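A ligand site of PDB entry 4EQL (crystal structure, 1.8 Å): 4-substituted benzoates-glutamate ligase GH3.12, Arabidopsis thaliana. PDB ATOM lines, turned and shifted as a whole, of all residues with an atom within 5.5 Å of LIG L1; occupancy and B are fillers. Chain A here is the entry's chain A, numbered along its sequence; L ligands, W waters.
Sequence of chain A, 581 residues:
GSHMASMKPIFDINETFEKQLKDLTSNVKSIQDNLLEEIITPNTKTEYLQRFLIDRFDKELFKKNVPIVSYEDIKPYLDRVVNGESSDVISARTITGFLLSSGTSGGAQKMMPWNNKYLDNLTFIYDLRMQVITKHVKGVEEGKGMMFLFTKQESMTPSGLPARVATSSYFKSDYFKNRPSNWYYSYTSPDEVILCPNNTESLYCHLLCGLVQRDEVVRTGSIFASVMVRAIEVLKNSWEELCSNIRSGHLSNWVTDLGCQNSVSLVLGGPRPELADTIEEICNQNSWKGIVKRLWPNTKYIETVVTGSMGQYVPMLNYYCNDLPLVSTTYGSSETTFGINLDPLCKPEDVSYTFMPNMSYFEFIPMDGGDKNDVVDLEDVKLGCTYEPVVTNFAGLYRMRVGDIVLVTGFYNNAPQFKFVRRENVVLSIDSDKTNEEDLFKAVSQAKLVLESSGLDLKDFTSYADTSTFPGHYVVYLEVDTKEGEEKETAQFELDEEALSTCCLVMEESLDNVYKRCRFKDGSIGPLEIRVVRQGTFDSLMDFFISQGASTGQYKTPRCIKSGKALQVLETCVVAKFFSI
Merely in contact with LIG L1: Val 305, Gly 308, Tyr 331, Gly 332, Ser 333, Phe 420 and Lys 434. Hydrophobic or aromatic side chains within 4 Å of LIG L1: Val 305, Tyr 331, Tyr 353 and Phe 420. Of the 24 residues printed, 15 come within 4 Å of LIG L1. The nearest printed residue that does not touch LIG L1 is Phe 224 (4.1 Å).
The side-chain carboxylate (OD1) of Asp 404 lies within salt-bridge range of the guanidinium group (NH1) of Arg 423 (3.0 Å). The side-chain carboxylate of Asp 404 sits at hydrogen-bond distance from the side-chain hydroxyl of Tyr 331. OG of Ser 102 is in hydrogen-bond range of NZ of Lys 434 (2.9 Å). N of Gly 103 lies within hydrogen-bond range of OG of Ser 101 (3.0 Å). OH of Tyr 353 is in hydrogen-bond range of OG of Ser 328. The backbone carbonyl oxygen of Val 402 sits at hydrogen-bond distance from the guanidinium group of Arg 423. The backbone NH (N) of Phe 338 sits at hydrogen-bond distance from the backbone carbonyl oxygen (O) of Tyr 331 (2.9 Å). The side-chain hydroxyl (OG) of Ser 333 lies within hydrogen-bond range of the side-chain carboxylate (OE1) of Glu 335, 2.6 Å away.
The side-chain hydroxyl (OG1) of Thr 307 is in hydrogen-bond range of a nitrogen (N4) of LIG L1, 2.7 Å away. The side-chain carboxylate of Asp 404 is in hydrogen-bond range of an oxygen (O7) of LIG L1, at 2.7 Å. The backbone NH (N) of Ser 102 lies within hydrogen-bond range of an oxygen (O3) of LIG L1 (2.9 Å). The side-chain hydroxyl (OG) of Ser 102 lies within hydrogen-bond range of an oxygen (O3) of LIG L1, at 2.7 Å. The backbone carbonyl oxygen (O) of Thr 330 is in hydrogen-bond range of a nitrogen (N3) of LIG L1, 2.8 Å away. O2 of LIG L1 sits at hydrogen-bond distance from OG of Ser 101 (2.9 Å). O2 of LIG L1 is in hydrogen-bond range of N of Ser 334 (3.1 Å). The side-chain hydroxyl (OG) of Ser 334 is in hydrogen-bond range of an oxygen (O2) of LIG L1, 2.9 Å away. The side-chain hydroxyl of Tyr 353 is in hydrogen-bond range of a nitrogen (N3) of LIG L1 (3.1 Å). An oxygen (O6) of LIG L1 lies within hydrogen-bond range of the guanidinium group of Arg 423.
Water W1 lies within hydrogen-bond range of a nitrogen (N5) of LIG L1 and the backbone NH (N) of Ser 309. Water W4 bridges the side-chain amino group of Lys 434 (3.1 Å) and an oxygen (O5) of LIG L1 (3.3 Å). Water W3 lies within hydrogen-bond range of O of Leu 100 (2.9 Å), N of Ser 102 (3.2 Å) and O3 of LIG L1 (3.3 Å). Water W2 lies within hydrogen-bond range of the backbone NH of Ala 166 (2.7 Å), the backbone carbonyl oxygen of Leu 100 (2.8 Å), the side-chain hydroxyl of Ser 334 (3.1 Å) and an oxygen (O1) of LIG L1 (3.5 Å).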
ATOM      1  N   LEU A 100     -11.316 -30.660   3.161  1.00  0.00           N
ATOM      2  CA  LEU A 100     -11.738 -29.604   2.256  1.00  0.00           C
ATOM      3  C   LEU A 100     -10.750 -28.444   2.323  1.00  0.00           C
ATOM      4  O   LEU A 100     -10.573 -27.824   3.370  1.00  0.00           O
ATOM      5  CB  LEU A 100     -13.134 -29.126   2.653  1.00  0.00           C
ATOM      6  CG  LEU A 100     -14.285 -30.093   2.360  1.00  0.00           C
ATOM      7  CD1 LEU A 100     -15.522 -29.696   3.138  1.00  0.00           C
ATOM      8  CD2 LEU A 100     -14.567 -30.124   0.862  1.00  0.00           C
ATOM      9  N   SER A 101     -10.112 -28.132   1.214  1.00  0.00           N
ATOM     10  CA  SER A 101      -9.153 -27.049   1.191  1.00  0.00           C
ATOM     11  C   SER A 101      -9.875 -25.737   0.842  1.00  0.00           C
ATOM     12  O   SER A 101     -10.834 -25.749   0.083  1.00  0.00           O
ATOM     13  CB  SER A 101      -8.052 -27.349   0.169  1.00  0.00           C
ATOM     14  OG  SER A 101      -7.204 -26.223  -0.007  1.00  0.00           O
ATOM     15  N   SER A 102      -9.407 -24.628   1.411  1.00  0.00           N
ATOM     16  CA  SER A 102      -9.948 -23.324   1.045  1.00  0.00           C
ATOM     17  C   SER A 102      -9.536 -23.009  -0.383  1.00  0.00           C
ATOM     18  O   SER A 102     -10.176 -22.212  -1.069  1.00  0.00           O
ATOM     19  CB  SER A 102      -9.462 -22.232   2.003  1.00  0.00           C
ATOM     20  OG  SER A 102      -8.046 -22.190   2.062  1.00  0.00           O
ATOM     21  N   GLY A 103      -8.464 -23.662  -0.832  1.00  0.00           N
ATOM     22  CA  GLY A 103      -8.020 -23.546  -2.199  1.00  0.00           C
ATOM     23  C   GLY A 103      -8.993 -24.226  -3.132  1.00  0.00           C
ATOM     24  O   GLY A 103      -9.532 -25.280  -2.816  1.00  0.00           O
ATOM     25  N   ALA A 166      -9.713 -28.915   8.022  1.00  0.00           N
ATOM     26  CA  ALA A 166      -8.707 -29.499   8.902  1.00  0.00           C
ATOM     27  C   ALA A 166      -9.081 -29.524  10.385  1.00  0.00           C
ATOM     28  O   ALA A 166      -9.099 -30.566  11.024  1.00  0.00           O
ATOM     29  CB  ALA A 166      -7.347 -28.812   8.710  1.00  0.00           C
ATOM     30  N   PHE A 224      -7.322 -18.003  12.886  1.00  0.00           N
ATOM     31  CA  PHE A 224      -6.887 -16.858  12.100  1.00  0.00           C
ATOM     32  C   PHE A 224      -7.365 -15.524  12.666  1.00  0.00           C
ATOM     33  O   PHE A 224      -8.438 -15.438  13.284  1.00  0.00           O
ATOM     34  CB  PHE A 224      -7.355 -17.010  10.642  1.00  0.00           C
ATOM     35  CG  PHE A 224      -6.762 -18.187   9.940  1.00  0.00           C
ATOM     36  CD1 PHE A 224      -5.444 -18.171   9.507  1.00  0.00           C
ATOM     37  CD2 PHE A 224      -7.514 -19.338   9.736  1.00  0.00           C
ATOM     38  CE1 PHE A 224      -4.879 -19.270   8.866  1.00  0.00           C
ATOM     39  CE2 PHE A 224      -6.961 -20.452   9.097  1.00  0.00           C
ATOM     40  CZ  PHE A 224      -5.643 -20.413   8.656  1.00  0.00           C
ATOM     41  N   VAL A 305      -3.216 -16.501  14.098  1.00  0.00           N
ATOM     42  CA  VAL A 305      -2.329 -16.272  12.952  1.00  0.00           C
ATOM     43  C   VAL A 305      -2.471 -14.852  12.439  1.00  0.00           C
ATOM     44  O   VAL A 305      -3.584 -14.390  12.141  1.00  0.00           O
ATOM     45  CB  VAL A 305      -2.592 -17.275  11.821  1.00  0.00           C
ATOM     46  CG1 VAL A 305      -1.977 -16.781  10.499  1.00  0.00           C
ATOM     47  CG2 VAL A 305      -2.054 -18.636  12.211  1.00  0.00           C
ATOM     48  N   THR A 307      -0.079 -13.695   9.989  1.00  0.00           N
ATOM     49  CA  THR A 307       0.789 -13.666   8.817  1.00  0.00           C
ATOM     50  C   THR A 307      -0.005 -13.822   7.527  1.00  0.00           C
ATOM     51  O   THR A 307      -1.216 -14.096   7.557  1.00  0.00           O
ATOM     52  CB  THR A 307       1.876 -14.752   8.931  1.00  0.00           C
ATOM     53  OG1 THR A 307       1.262 -15.983   9.360  1.00  0.00           O
ATOM     54  CG2 THR A 307       2.897 -14.347   9.984  1.00  0.00           C
ATOM     55  N   GLY A 308       0.651 -13.626   6.390  1.00  0.00           N
ATOM     56  CA  GLY A 308      -0.041 -13.643   5.111  1.00  0.00           C
ATOM     57  C   GLY A 308      -1.162 -12.613   5.036  1.00  0.00           C
ATOM     58  O   GLY A 308      -1.000 -11.458   5.451  1.00  0.00           O
ATOM     59  N   SER A 309      -2.315 -13.018   4.529  1.00  0.00           N
ATOM     60  CA  SER A 309      -3.422 -12.074   4.356  1.00  0.00           C
ATOM     61  C   SER A 309      -3.957 -11.598   5.699  1.00  0.00           C
ATOM     62  O   SER A 309      -4.624 -10.557   5.789  1.00  0.00           O
ATOM     63  CB  SER A 309      -4.548 -12.716   3.542  1.00  0.00           C
ATOM     64  OG  SER A 309      -5.025 -13.890   4.175  1.00  0.00           O
ATOM     65  N   SER A 328       1.536 -15.829  16.819  1.00  0.00           N
ATOM     66  CA  SER A 328       1.180 -16.508  15.597  1.00  0.00           C
ATOM     67  C   SER A 328       1.992 -17.806  15.553  1.00  0.00           C
ATOM     68  O   SER A 328       3.179 -17.769  15.227  1.00  0.00           O
ATOM     69  CB  SER A 328       1.556 -15.600  14.431  1.00  0.00           C
ATOM     70  OG  SER A 328       0.947 -15.986  13.218  1.00  0.00           O
ATOM     71  N   THR A 330       1.463 -21.235  14.092  1.00  0.00           N
ATOM     72  CA  THR A 330       1.415 -22.423  13.244  1.00  0.00           C
ATOM     73  C   THR A 330       1.111 -22.123  11.790  1.00  0.00           C
ATOM     74  O   THR A 330       0.285 -21.275  11.485  1.00  0.00           O
ATOM     75  CB  THR A 330       0.355 -23.419  13.792  1.00  0.00           C
ATOM     76  OG1 THR A 330       0.613 -23.671  15.175  1.00  0.00           O
ATOM     77  CG2 THR A 330       0.407 -24.763  13.038  1.00  0.00           C
ATOM     78  N   TYR A 331       1.807 -22.844  10.909  1.00  0.00           N
ATOM     79  CA  TYR A 331       1.583 -22.772   9.469  1.00  0.00           C
ATOM     80  C   TYR A 331       1.202 -24.193   9.041  1.00  0.00           C
ATOM     81  O   TYR A 331       1.936 -25.141   9.325  1.00  0.00           O
ATOM     82  CB  TYR A 331       2.862 -22.297   8.778  1.00  0.00           C
ATOM     83  CG  TYR A 331       2.863 -22.383   7.264  1.00  0.00           C
ATOM     84  CD1 TYR A 331       1.699 -22.236   6.514  1.00  0.00           C
ATOM     85  CD2 TYR A 331       4.057 -22.612   6.590  1.00  0.00           C
ATOM     86  CE1 TYR A 331       1.720 -22.318   5.126  1.00  0.00           C
ATOM     87  CE2 TYR A 331       4.099 -22.694   5.214  1.00  0.00           C
ATOM     88  CZ  TYR A 331       2.936 -22.544   4.486  1.00  0.00           C
ATOM     89  OH  TYR A 331       3.013 -22.639   3.115  1.00  0.00           O
ATOM     90  N   GLY A 332       0.053 -24.337   8.400  1.00  0.00           N
ATOM     91  CA  GLY A 332      -0.445 -25.657   8.019  1.00  0.00           C
ATOM     92  C   GLY A 332      -1.393 -25.590   6.836  1.00  0.00           C
ATOM     93  O   GLY A 332      -1.895 -24.516   6.514  1.00  0.00           O
ATOM     94  N   SER A 333      -1.645 -26.737   6.209  1.00  0.00           N
ATOM     95  CA  SER A 333      -2.542 -26.798   5.070  1.00  0.00           C
ATOM     96  C   SER A 333      -3.230 -28.151   5.057  1.00  0.00           C
ATOM     97  O   SER A 333      -2.922 -29.013   5.891  1.00  0.00           O
ATOM     98  CB  SER A 333      -1.782 -26.626   3.760  1.00  0.00           C
ATOM     99  OG  SER A 333      -0.939 -27.750   3.532  1.00  0.00           O
ATOM    100  N   SER A 334      -4.137 -28.340   4.100  1.00  0.00           N
ATOM    101  CA  SER A 334      -4.847 -29.599   3.947  1.00  0.00           C
ATOM    102  C   SER A 334      -3.911 -30.740   3.542  1.00  0.00           C
ATOM    103  O   SER A 334      -4.247 -31.925   3.688  1.00  0.00           O
ATOM    104  CB  SER A 334      -5.976 -29.454   2.925  1.00  0.00           C
ATOM    105  OG  SER A 334      -6.890 -28.461   3.350  1.00  0.00           O
ATOM    106  N   GLU A 335      -2.732 -30.406   3.015  1.00  0.00           N
ATOM    107  CA  GLU A 335      -1.742 -31.427   2.683  1.00  0.00           C
ATOM    108  C   GLU A 335      -0.987 -31.944   3.909  1.00  0.00           C
ATOM    109  O   GLU A 335      -0.670 -33.131   3.995  1.00  0.00           O
ATOM    110  CB  GLU A 335      -0.716 -30.908   1.669  1.00  0.00           C
ATOM    111  CG  GLU A 335      -1.262 -30.622   0.299  1.00  0.00           C
ATOM    112  CD  GLU A 335      -1.744 -29.191   0.151  1.00  0.00           C
ATOM    113  OE1 GLU A 335      -1.614 -28.403   1.105  1.00  0.00           O
ATOM    114  OE2 GLU A 335      -2.261 -28.848  -0.934  1.00  0.00           O
ATOM    115  N   PHE A 338       2.869 -27.776   8.565  1.00  0.00           N
ATOM    116  CA  PHE A 338       4.247 -27.525   8.178  1.00  0.00           C
ATOM    117  C   PHE A 338       5.156 -27.349   9.398  1.00  0.00           C
ATOM    118  O   PHE A 338       6.155 -28.059   9.549  1.00  0.00           O
ATOM    119  CB  PHE A 338       4.352 -26.303   7.254  1.00  0.00           C
ATOM    120  CG  PHE A 338       3.656 -26.485   5.926  1.00  0.00           C
ATOM    121  CD1 PHE A 338       4.177 -27.351   4.967  1.00  0.00           C
ATOM    122  CD2 PHE A 338       2.495 -25.780   5.625  1.00  0.00           C
ATOM    123  CE1 PHE A 338       3.552 -27.519   3.743  1.00  0.00           C
ATOM    124  CE2 PHE A 338       1.856 -25.929   4.377  1.00  0.00           C
ATOM    125  CZ  PHE A 338       2.383 -26.809   3.446  1.00  0.00           C
ATOM    126  N   TYR A 353       8.255 -19.407  10.283  1.00  0.00           N
ATOM    127  CA  TYR A 353       7.811 -20.732  10.720  1.00  0.00           C
ATOM    128  C   TYR A 353       8.906 -21.749  10.420  1.00  0.00           C
ATOM    129  O   TYR A 353       9.406 -21.821   9.307  1.00  0.00           O
ATOM    130  CB  TYR A 353       6.521 -21.136   9.976  1.00  0.00           C
ATOM    131  CG  TYR A 353       5.387 -20.189  10.282  1.00  0.00           C
ATOM    132  CD1 TYR A 353       4.693 -20.287  11.486  1.00  0.00           C
ATOM    133  CD2 TYR A 353       5.022 -19.183   9.398  1.00  0.00           C
ATOM    134  CE1 TYR A 353       3.640 -19.411  11.787  1.00  0.00           C
ATOM    135  CE2 TYR A 353       3.985 -18.293   9.705  1.00  0.00           C
ATOM    136  CZ  TYR A 353       3.312 -18.408  10.897  1.00  0.00           C
ATOM    137  OH  TYR A 353       2.292 -17.540  11.216  1.00  0.00           O
ATOM    138  N   VAL A 402       2.151 -27.255  -3.283  1.00  0.00           N
ATOM    139  CA  VAL A 402       1.218 -26.687  -2.312  1.00  0.00           C
ATOM    140  C   VAL A 402       0.596 -25.380  -2.795  1.00  0.00           C
ATOM    141  O   VAL A 402      -0.494 -25.001  -2.363  1.00  0.00           O
ATOM    142  CB  VAL A 402       1.941 -26.458  -0.955  1.00  0.00           C
ATOM    143  CG1 VAL A 402       1.104 -25.608  -0.034  1.00  0.00           C
ATOM    144  CG2 VAL A 402       2.257 -27.810  -0.308  1.00  0.00           C
ATOM    145  N   ASP A 404       1.760 -22.388  -2.271  1.00  0.00           N
ATOM    146  CA  ASP A 404       2.149 -21.269  -1.421  1.00  0.00           C
ATOM    147  C   ASP A 404       3.536 -20.803  -1.819  1.00  0.00           C
ATOM    148  O   ASP A 404       4.285 -21.537  -2.447  1.00  0.00           O
ATOM    149  CB  ASP A 404       2.179 -21.677   0.071  1.00  0.00           C
ATOM    150  CG  ASP A 404       0.813 -21.830   0.680  1.00  0.00           C
ATOM    151  OD1 ASP A 404      -0.165 -21.207   0.205  1.00  0.00           O
ATOM    152  OD2 ASP A 404       0.712 -22.590   1.659  1.00  0.00           O
ATOM    153  N   PHE A 420       5.973 -16.676   5.486  1.00  0.00           N
ATOM    154  CA  PHE A 420       4.913 -16.906   4.513  1.00  0.00           C
ATOM    155  C   PHE A 420       4.747 -15.654   3.660  1.00  0.00           C
ATOM    156  O   PHE A 420       4.506 -14.569   4.176  1.00  0.00           O
ATOM    157  CB  PHE A 420       3.597 -17.255   5.210  1.00  0.00           C
ATOM    158  CG  PHE A 420       2.474 -17.550   4.243  1.00  0.00           C
ATOM    159  CD1 PHE A 420       2.248 -18.837   3.801  1.00  0.00           C
ATOM    160  CD2 PHE A 420       1.659 -16.525   3.764  1.00  0.00           C
ATOM    161  CE1 PHE A 420       1.226 -19.108   2.904  1.00  0.00           C
ATOM    162  CE2 PHE A 420       0.639 -16.786   2.856  1.00  0.00           C
ATOM    163  CZ  PHE A 420       0.416 -18.084   2.434  1.00  0.00           C
ATOM    164  N   ARG A 423      -0.248 -16.931  -1.009  1.00  0.00           N
ATOM    165  CA  ARG A 423      -0.726 -18.066  -1.799  1.00  0.00           C
ATOM    166  C   ARG A 423      -0.718 -17.618  -3.257  1.00  0.00           C
ATOM    167  O   ARG A 423      -1.246 -16.568  -3.616  1.00  0.00           O
ATOM    168  CB  ARG A 423      -2.123 -18.505  -1.359  1.00  0.00           C
ATOM    169  CG  ARG A 423      -2.594 -19.736  -2.102  1.00  0.00           C
ATOM    170  CD  ARG A 423      -3.665 -20.479  -1.317  1.00  0.00           C
ATOM    171  NE  ARG A 423      -4.029 -21.725  -1.978  1.00  0.00           N
ATOM    172  CZ  ARG A 423      -3.340 -22.861  -1.850  1.00  0.00           C
ATOM    173  NH1 ARG A 423      -2.245 -22.898  -1.105  1.00  0.00           N
ATOM    174  NH2 ARG A 423      -3.733 -23.960  -2.495  1.00  0.00           N
ATOM    175  N   LYS A 434     -10.126 -17.343  -0.531  1.00  0.00           N
ATOM    176  CA  LYS A 434      -8.906 -17.032  -1.269  1.00  0.00           C
ATOM    177  C   LYS A 434      -9.221 -16.952  -2.756  1.00  0.00           C
ATOM    178  O   LYS A 434      -8.978 -17.899  -3.505  1.00  0.00           O
ATOM    179  CB  LYS A 434      -7.825 -18.079  -1.002  1.00  0.00           C
ATOM    180  CG  LYS A 434      -7.263 -18.037   0.406  1.00  0.00           C
ATOM    181  CD  LYS A 434      -6.240 -19.138   0.623  1.00  0.00           C
ATOM    182  CE  LYS A 434      -5.860 -19.266   2.095  1.00  0.00           C
ATOM    183  NZ  LYS A 434      -7.034 -19.646   2.933  1.00  0.00           N
HETATM  184  P1  LIG L   1      -5.823 -25.384   3.401  1.00  0.00           P
HETATM  185  O1  LIG L   1      -6.145 -26.037   4.720  1.00  0.00           O
HETATM  186  O2  LIG L   1      -5.434 -26.262   2.232  1.00  0.00           O
HETATM  187  O3  LIG L   1      -6.993 -24.508   3.045  1.00  0.00           O
HETATM  188  O4  LIG L   1      -4.709 -24.255   3.605  1.00  0.00           O
HETATM  189  C1  LIG L   1      -5.102 -22.893   3.583  1.00  0.00           C
HETATM  190  C2  LIG L   1      -3.959 -21.925   3.336  1.00  0.00           C
HETATM  191  O5  LIG L   1      -3.939 -20.946   4.394  1.00  0.00           O
HETATM  192  C3  LIG L   1      -2.535 -22.436   3.365  1.00  0.00           C
HETATM  193  O6  LIG L   1      -2.172 -23.216   2.235  1.00  0.00           O
HETATM  194  C4  LIG L   1      -1.798 -21.110   3.428  1.00  0.00           C
HETATM  195  O7  LIG L   1      -1.881 -20.432   2.173  1.00  0.00           O
HETATM  196  C5  LIG L   1      -2.663 -20.352   4.424  1.00  0.00           C
HETATM  197  N1  LIG L   1      -2.120 -20.463   5.792  1.00  0.00           N
HETATM  198  C6  LIG L   1      -2.098 -21.516   6.633  1.00  0.00           C
HETATM  199  N2  LIG L   1      -1.388 -21.201   7.755  1.00  0.00           N
HETATM  200  C7  LIG L   1      -0.933 -19.932   7.580  1.00  0.00           C
HETATM  201  C8  LIG L   1      -0.123 -18.966   8.326  1.00  0.00           C
HETATM  202  N3  LIG L   1       0.377 -19.280   9.534  1.00  0.00           N
HETATM  203  N4  LIG L   1       0.112 -17.758   7.762  1.00  0.00           N
HETATM  204  C9  LIG L   1      -0.348 -17.411   6.553  1.00  0.00           C
HETATM  205  N5  LIG L   1      -1.099 -18.247   5.803  1.00  0.00           N
HETATM  206  C10 LIG L   1      -1.402 -19.470   6.272  1.00  0.00           C
HETATM  207  C1  LG2 L   2      -4.214 -24.993  13.807  1.00  0.00           C
HETATM  208  O1  LG2 L   2      -4.085 -24.372  14.888  1.00  0.00           O
HETATM  209  O2  LG2 L   2      -4.737 -26.149  13.832  1.00  0.00           O
HETATM  210  C2  LG2 L   2      -3.710 -24.415  12.515  1.00  0.00           C
HETATM  211  C3  LG2 L   2      -3.801 -25.152  11.342  1.00  0.00           C
HETATM  212  C4  LG2 L   2      -3.372 -24.620  10.132  1.00  0.00           C
HETATM  213  C5  LG2 L   2      -2.853 -23.339  10.097  1.00  0.00           C
HETATM  214  C6  LG2 L   2      -2.767 -22.588  11.264  1.00  0.00           C
HETATM  215  C7  LG2 L   2      -3.186 -23.126  12.479  1.00  0.00           C
HETATM  216  O3  LG2 L   2      -4.313 -26.438  11.373  1.00  0.00           O
HETATM  217  O   HOH W   1      -2.596 -16.343   3.973  1.00  0.00           O
HETATM  218  O   HOH W   2      -8.891 -27.957   5.633  1.00  0.00           O
HETATM  219  O   HOH W   3      -9.860 -25.264   4.500  1.00  0.00           O
HETATM  220  O   HOH W   4      -6.997 -21.176   5.649  1.00  0.00           O
